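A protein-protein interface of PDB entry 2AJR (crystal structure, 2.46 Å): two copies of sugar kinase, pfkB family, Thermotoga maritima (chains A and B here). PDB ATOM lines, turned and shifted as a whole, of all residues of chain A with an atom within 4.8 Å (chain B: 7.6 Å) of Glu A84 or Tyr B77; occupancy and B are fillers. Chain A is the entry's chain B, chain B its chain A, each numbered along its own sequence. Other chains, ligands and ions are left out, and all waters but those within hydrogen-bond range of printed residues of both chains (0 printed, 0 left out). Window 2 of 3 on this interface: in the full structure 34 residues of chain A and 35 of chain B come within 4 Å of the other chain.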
ATOM      1  N   TYR A  77      27.480  14.881  25.075  1.00  0.00           N
ATOM      2  CA  TYR A  77      27.304  13.804  25.994  1.00  0.00           C
ATOM      3  C   TYR A  77      26.660  12.608  25.318  1.00  0.00           C
ATOM      4  O   TYR A  77      27.067  11.475  25.549  1.00  0.00           O
ATOM      5  CB  TYR A  77      26.465  14.303  27.154  1.00  0.00           C
ATOM      6  CG  TYR A  77      26.519  13.412  28.350  1.00  0.00           C
ATOM      7  CD1 TYR A  77      27.659  13.356  29.148  1.00  0.00           C
ATOM      8  CD2 TYR A  77      25.422  12.627  28.691  1.00  0.00           C
ATOM      9  CE1 TYR A  77      27.701  12.541  30.255  1.00  0.00           C
ATOM     10  CE2 TYR A  77      25.448  11.806  29.793  1.00  0.00           C
ATOM     11  CZ  TYR A  77      26.582  11.763  30.575  1.00  0.00           C
ATOM     12  OH  TYR A  77      26.581  10.933  31.661  1.00  0.00           O
ATOM     13  N   LYS A  80      29.456  10.893  23.627  1.00  0.00           N
ATOM     14  CA  LYS A  80      30.185  10.008  24.535  1.00  0.00           C
ATOM     15  C   LYS A  80      29.505   8.662  24.655  1.00  0.00           C
ATOM     16  O   LYS A  80      30.177   7.625  24.694  1.00  0.00           O
ATOM     17  CB  LYS A  80      30.280  10.622  25.935  1.00  0.00           C
ATOM     18  CG  LYS A  80      31.094   9.815  26.950  1.00  0.00           C
ATOM     19  CD  LYS A  80      30.851  10.363  28.355  1.00  0.00           C
ATOM     20  CE  LYS A  80      31.647   9.636  29.435  1.00  0.00           C
ATOM     21  NZ  LYS A  80      31.832  10.453  30.665  1.00  0.00           N
ATOM     22  N   ILE A  81      28.175   8.680  24.725  1.00  0.00           N
ATOM     23  CA  ILE A  81      27.403   7.468  24.944  1.00  0.00           C
ATOM     24  C   ILE A  81      27.486   6.576  23.712  1.00  0.00           C
ATOM     25  O   ILE A  81      27.734   5.369  23.820  1.00  0.00           O
ATOM     26  CB  ILE A  81      25.933   7.802  25.284  1.00  0.00           C
ATOM     27  CG1 ILE A  81      25.843   8.541  26.618  1.00  0.00           C
ATOM     28  CG2 ILE A  81      25.073   6.546  25.355  1.00  0.00           C
ATOM     29  CD1 ILE A  81      24.499   9.233  26.833  1.00  0.00           C
ATOM     30  N   LEU A  82      27.301   7.174  22.540  1.00  0.00           N
ATOM     31  CA  LEU A  82      27.393   6.431  21.301  1.00  0.00           C
ATOM     32  C   LEU A  82      28.745   5.746  21.193  1.00  0.00           C
ATOM     33  O   LEU A  82      28.824   4.558  20.897  1.00  0.00           O
ATOM     34  CB  LEU A  82      27.187   7.353  20.106  1.00  0.00           C
ATOM     35  CG  LEU A  82      27.103   6.656  18.742  1.00  0.00           C
ATOM     36  CD1 LEU A  82      26.208   7.447  17.806  1.00  0.00           C
ATOM     37  CD2 LEU A  82      28.492   6.462  18.140  1.00  0.00           C
ATOM     38  N   VAL A  83      29.804   6.505  21.452  1.00  0.00           N
ATOM     39  CA  VAL A  83      31.155   6.011  21.308  1.00  0.00           C
ATOM     40  C   VAL A  83      31.451   4.942  22.332  1.00  0.00           C
ATOM     41  O   VAL A  83      32.047   3.914  21.989  1.00  0.00           O
ATOM     42  CB  VAL A  83      32.193   7.143  21.415  1.00  0.00           C
ATOM     43  CG1 VAL A  83      33.608   6.579  21.439  1.00  0.00           C
ATOM     44  CG2 VAL A  83      32.021   8.098  20.238  1.00  0.00           C
ATOM     45  N   GLU A  84      31.039   5.165  23.583  1.00  0.00           N
ATOM     46  CA  GLU A  84      31.321   4.180  24.646  1.00  0.00           C
ATOM     47  C   GLU A  84      30.560   2.889  24.354  1.00  0.00           C
ATOM     48  O   GLU A  84      31.117   1.803  24.432  1.00  0.00           O
ATOM     49  CB  GLU A  84      31.017   4.733  26.058  1.00  0.00           C
ATOM     50  CG  GLU A  84      32.178   5.556  26.669  1.00  0.00           C
ATOM     51  CD  GLU A  84      31.831   6.226  28.019  1.00  0.00           C
ATOM     52  OE1 GLU A  84      30.730   5.991  28.580  1.00  0.00           O
ATOM     53  OE2 GLU A  84      32.675   6.990  28.538  1.00  0.00           O
ATOM     54  N   GLU A  85      29.299   3.024  23.952  1.00  0.00           N
ATOM     55  CA  GLU A  85      28.475   1.863  23.606  1.00  0.00           C
ATOM     56  C   GLU A  85      28.968   1.125  22.359  1.00  0.00           C
ATOM     57  O   GLU A  85      28.990  -0.095  22.326  1.00  0.00           O
ATOM     58  CB  GLU A  85      27.004   2.275  23.458  1.00  0.00           C
ATOM     59  CG  GLU A  85      26.345   2.692  24.794  1.00  0.00           C
ATOM     60  CD  GLU A  85      26.485   1.619  25.867  1.00  0.00           C
ATOM     61  OE1 GLU A  85      26.149   0.448  25.567  1.00  0.00           O
ATOM     62  OE2 GLU A  85      26.952   1.940  26.988  1.00  0.00           O
ATOM     63  N   LEU A  86      29.383   1.858  21.340  1.00  0.00           N
ATOM     64  CA  LEU A  86      29.842   1.231  20.111  1.00  0.00           C
ATOM     65  C   LEU A  86      31.077   0.380  20.363  1.00  0.00           C
ATOM     66  O   LEU A  86      31.206  -0.706  19.813  1.00  0.00           O
ATOM     67  CB  LEU A  86      30.152   2.294  19.058  1.00  0.00           C
ATOM     68  CG  LEU A  86      30.513   1.763  17.678  1.00  0.00           C
ATOM     69  CD1 LEU A  86      29.490   0.750  17.209  1.00  0.00           C
ATOM     70  CD2 LEU A  86      30.639   2.928  16.714  1.00  0.00           C
ATOM     71  N   ARG A  87      31.981   0.889  21.195  1.00  0.00           N
ATOM     72  CA  ARG A  87      33.204   0.178  21.537  1.00  0.00           C
ATOM     73  C   ARG A  87      32.869  -1.121  22.258  1.00  0.00           C
ATOM     74  O   ARG A  87      33.536  -2.133  22.052  1.00  0.00           O
ATOM     75  CB  ARG A  87      34.124   1.049  22.400  1.00  0.00           C
ATOM     76  CG  ARG A  87      34.900   2.151  21.626  1.00  0.00           C
ATOM     77  CD  ARG A  87      35.809   2.955  22.571  1.00  0.00           C
ATOM     78  NE  ARG A  87      36.391   4.163  21.963  1.00  0.00           N
ATOM     79  CZ  ARG A  87      36.374   5.396  22.496  1.00  0.00           C
ATOM     80  NH1 ARG A  87      35.795   5.663  23.674  1.00  0.00           N
ATOM     81  NH2 ARG A  87      36.940   6.394  21.829  1.00  0.00           N
ATOM     82  N   LYS A  88      31.829  -1.094  23.098  1.00  0.00           N
ATOM     83  CA  LYS A  88      31.420  -2.283  23.859  1.00  0.00           C
ATOM     84  C   LYS A  88      30.873  -3.435  22.991  1.00  0.00           C
ATOM     85  O   LYS A  88      30.901  -4.583  23.413  1.00  0.00           O
ATOM     86  CB  LYS A  88      30.419  -1.885  24.959  1.00  0.00           C
ATOM     87  CG  LYS A  88      31.106  -1.141  26.140  1.00  0.00           C
ATOM     88  CD  LYS A  88      30.217  -0.867  27.378  1.00  0.00           C
ATOM     89  CE  LYS A  88      30.940   0.114  28.324  1.00  0.00           C
ATOM     90  NZ  LYS A  88      30.582  -0.001  29.773  1.00  0.00           N
ATOM     91  N   LEU B  23      13.919  11.777  33.391  1.00  0.00           N
ATOM     92  CA  LEU B  23      14.110  12.839  32.421  1.00  0.00           C
ATOM     93  C   LEU B  23      12.897  12.859  31.505  1.00  0.00           C
ATOM     94  O   LEU B  23      12.567  11.859  30.889  1.00  0.00           O
ATOM     95  CB  LEU B  23      15.358  12.585  31.585  1.00  0.00           C
ATOM     96  CG  LEU B  23      16.646  12.858  32.338  1.00  0.00           C
ATOM     97  CD1 LEU B  23      17.814  12.203  31.635  1.00  0.00           C
ATOM     98  CD2 LEU B  23      16.837  14.357  32.448  1.00  0.00           C
ATOM     99  N   GLY B  75      20.631   6.971  38.457  1.00  0.00           N
ATOM    100  CA  GLY B  75      21.694   6.090  37.979  1.00  0.00           C
ATOM    101  C   GLY B  75      22.107   6.283  36.550  1.00  0.00           C
ATOM    102  O   GLY B  75      21.376   6.860  35.762  1.00  0.00           O
ATOM    103  N   GLY B  76      23.289   5.777  36.221  1.00  0.00           N
ATOM    104  CA  GLY B  76      23.805   5.800  34.854  1.00  0.00           C
ATOM    105  C   GLY B  76      23.928   7.155  34.185  1.00  0.00           C
ATOM    106  O   GLY B  76      24.017   8.189  34.843  1.00  0.00           O
ATOM    107  N   TYR B  77      23.933   7.128  32.857  1.00  0.00           N
ATOM    108  CA  TYR B  77      24.043   8.328  32.034  1.00  0.00           C
ATOM    109  C   TYR B  77      22.896   9.303  32.250  1.00  0.00           C
ATOM    110  O   TYR B  77      23.110  10.518  32.349  1.00  0.00           O
ATOM    111  CB  TYR B  77      24.058   7.955  30.554  1.00  0.00           C
ATOM    112  CG  TYR B  77      25.247   7.148  30.103  1.00  0.00           C
ATOM    113  CD1 TYR B  77      26.550   7.673  30.162  1.00  0.00           C
ATOM    114  CD2 TYR B  77      25.068   5.870  29.579  1.00  0.00           C
ATOM    115  CE1 TYR B  77      27.639   6.932  29.715  1.00  0.00           C
ATOM    116  CE2 TYR B  77      26.142   5.119  29.133  1.00  0.00           C
ATOM    117  CZ  TYR B  77      27.425   5.651  29.201  1.00  0.00           C
ATOM    118  OH  TYR B  77      28.467   4.871  28.745  1.00  0.00           O
ATOM    119  N   MET B  78      21.679   8.774  32.296  1.00  0.00           N
ATOM    120  CA  MET B  78      20.510   9.605  32.476  1.00  0.00           C
ATOM    121  C   MET B  78      20.554  10.235  33.859  1.00  0.00           C
ATOM    122  O   MET B  78      20.190  11.405  34.048  1.00  0.00           O
ATOM    123  CB  MET B  78      19.242   8.771  32.317  1.00  0.00           C
ATOM    124  CG  MET B  78      19.080   8.116  30.942  1.00  0.00           C
ATOM    125  SD  MET B  78      19.121   9.389  29.455  1.00  0.00           S
ATOM    126  CE  MET B  78      20.941   9.241  28.827  1.00  0.00           C
ATOM    127  N   GLY B  79      21.026   9.469  34.831  1.00  0.00           N
ATOM    128  CA  GLY B  79      21.153   9.995  36.171  1.00  0.00           C
ATOM    129  C   GLY B  79      22.030  11.225  36.196  1.00  0.00           C
ATOM    130  O   GLY B  79      21.675  12.219  36.820  1.00  0.00           O
ATOM    131  N   LYS B  80      23.167  11.162  35.511  1.00  0.00           N
ATOM    132  CA  LYS B  80      24.116  12.273  35.515  1.00  0.00           C
ATOM    133  C   LYS B  80      23.502  13.527  34.928  1.00  0.00           C
ATOM    134  O   LYS B  80      23.648  14.618  35.481  1.00  0.00           O
ATOM    135  CB  LYS B  80      25.397  11.934  34.732  1.00  0.00           C
ATOM    136  CG  LYS B  80      26.285  13.160  34.463  1.00  0.00           C
ATOM    137  CD  LYS B  80      27.767  12.794  34.246  1.00  0.00           C
ATOM    138  CE  LYS B  80      28.644  14.032  33.919  1.00  0.00           C
ATOM    139  NZ  LYS B  80      28.009  14.979  32.899  1.00  0.00           N
ATOM    140  N   ILE B  81      22.824  13.366  33.798  1.00  0.00           N
ATOM    141  CA  ILE B  81      22.142  14.470  33.174  1.00  0.00           C
ATOM    142  C   ILE B  81      21.119  15.057  34.139  1.00  0.00           C
ATOM    143  O   ILE B  81      21.052  16.270  34.309  1.00  0.00           O
ATOM    144  CB  ILE B  81      21.421  14.042  31.886  1.00  0.00           C
ATOM    145  CG1 ILE B  81      22.421  13.561  30.838  1.00  0.00           C
ATOM    146  CG2 ILE B  81      20.593  15.208  31.315  1.00  0.00           C
ATOM    147  CD1 ILE B  81      21.733  12.826  29.677  1.00  0.00           C
ATOM    148  N   LEU B  82      20.326  14.204  34.779  1.00  0.00           N
ATOM    149  CA  LEU B  82      19.263  14.696  35.677  1.00  0.00           C
ATOM    150  C   LEU B  82      19.834  15.583  36.771  1.00  0.00           C
ATOM    151  O   LEU B  82      19.344  16.691  36.988  1.00  0.00           O
ATOM    152  CB  LEU B  82      18.480  13.533  36.308  1.00  0.00           C
ATOM    153  CG  LEU B  82      17.184  13.863  37.049  1.00  0.00           C
ATOM    154  CD1 LEU B  82      16.061  12.899  36.641  1.00  0.00           C
ATOM    155  CD2 LEU B  82      17.364  13.845  38.547  1.00  0.00           C
ATOM    156  N   VAL B  83      20.887  15.115  37.441  1.00  0.00           N
ATOM    157  CA  VAL B  83      21.404  15.813  38.606  1.00  0.00           C
ATOM    158  C   VAL B  83      21.984  17.144  38.174  1.00  0.00           C
ATOM    159  O   VAL B  83      21.787  18.165  38.846  1.00  0.00           O
ATOM    160  CB  VAL B  83      22.460  14.962  39.385  1.00  0.00           C
ATOM    161  CG1 VAL B  83      23.144  15.780  40.470  1.00  0.00           C
ATOM    162  CG2 VAL B  83      21.798  13.737  39.994  1.00  0.00           C
ATOM    163  N   GLY B 102      22.394   1.148  36.920  1.00  0.00           N
ATOM    164  CA  GLY B 102      21.178   1.140  36.089  1.00  0.00           C
ATOM    165  C   GLY B 102      20.764   2.546  35.744  1.00  0.00           C
ATOM    166  O   GLY B 102      21.175   3.489  36.401  1.00  0.00           O
ATOM    167  N   GLU B 103      19.941   2.683  34.715  1.00  0.00           N
ATOM    168  CA  GLU B 103      19.608   3.990  34.172  1.00  0.00           C
ATOM    169  C   GLU B 103      18.362   4.622  34.787  1.00  0.00           C
ATOM    170  O   GLU B 103      17.322   3.976  34.905  1.00  0.00           O
ATOM    171  CB  GLU B 103      19.420   3.884  32.662  1.00  0.00           C
ATOM    172  CG  GLU B 103      20.708   3.533  31.911  1.00  0.00           C
ATOM    173  CD  GLU B 103      21.711   4.692  31.811  1.00  0.00           C
ATOM    174  OE1 GLU B 103      21.272   5.858  31.792  1.00  0.00           O
ATOM    175  OE2 GLU B 103      22.934   4.424  31.737  1.00  0.00           O
ATOM    176  N   THR B 104      18.477   5.888  35.170  1.00  0.00           N
ATOM    177  CA  THR B 104      17.311   6.685  35.454  1.00  0.00           C
ATOM    178  C   THR B 104      16.448   6.729  34.190  1.00  0.00           C
ATOM    179  O   THR B 104      16.954   6.913  33.092  1.00  0.00           O
ATOM    180  CB  THR B 104      17.690   8.098  35.868  1.00  0.00           C
ATOM    181  OG1 THR B 104      18.319   8.060  37.157  1.00  0.00           O
ATOM    182  CG2 THR B 104      16.433   8.997  35.929  1.00  0.00           C
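The side-chain hydroxyl (OH) of Tyr B77 lies within hydrogen-bond range of the side-chain carboxylate (OE1) of Glu A84, 2.5 Å away.
Tyr A77 touches its own counterpart, Tyr B77. Tyr A77 touches Lys B80, but with the chains exchanged Lys A80 does not touch Tyr B77 (4.8 Å). Tyr A77 touches Ile B81, and with the chains exchanged Ile A81 touches Tyr B77. 5 positions are printed for both chains.
Printed residues of chain B within 4 Å of Tyr A77: Tyr B77 (3.6 Å), Lys B80 (3.4 Å) and Ile B81 (3.7 Å). Of the printed residues of chain B, Ile A81 touches Tyr B77 (3.7 Å). Of chain B, only Tyr B77 (2.5 Å) comes within 4 Å of Glu A84. Of the printed residues of chain B, Glu A85 touches Tyr B77 (3.7 Å). Tyr B77 touches four residues of chain A. Printed residues of chain A within 4 Å of Lys B80: Tyr A77 (3.4 Å). The nearest printed residue of chain B that does not touch Glu A84 is Glu B103 (8.6 Å). The nearest printed residue of chain A that does not touch Tyr B77 is Lys A80 (4.8 Å).
The backbone NH (N) of Tyr B77 lies within hydrogen-bond range of the side-chain carboxylate (OE2) of Glu B103.
Of the 13 printed residues of chain B, 3 touch a printed residue of chain A. Hydrophobic or aromatic side chains of chain B within 4 Å of the printed part of chain A: Tyr B77 and Ile B81. Of the 10 printed residues of chain A, 4 touch a printed residue of chain B. Hydrophobic or aromatic side chains of chain A that line the printed part of chain B: Tyr A77 and Ile A81. Among the printed residues, 6 pairs touch across the chains.
Among the printed residues, merely in contact across the chains: Tyr A77 with Tyr B77 (3.6 Å), Tyr A77 with Lys B80 (3.4 Å), Tyr A77 with Ile B81 (3.7 Å), Ile A81 with Tyr B77 (3.7 Å) and Glu A85 with Tyr B77 (3.7 Å).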
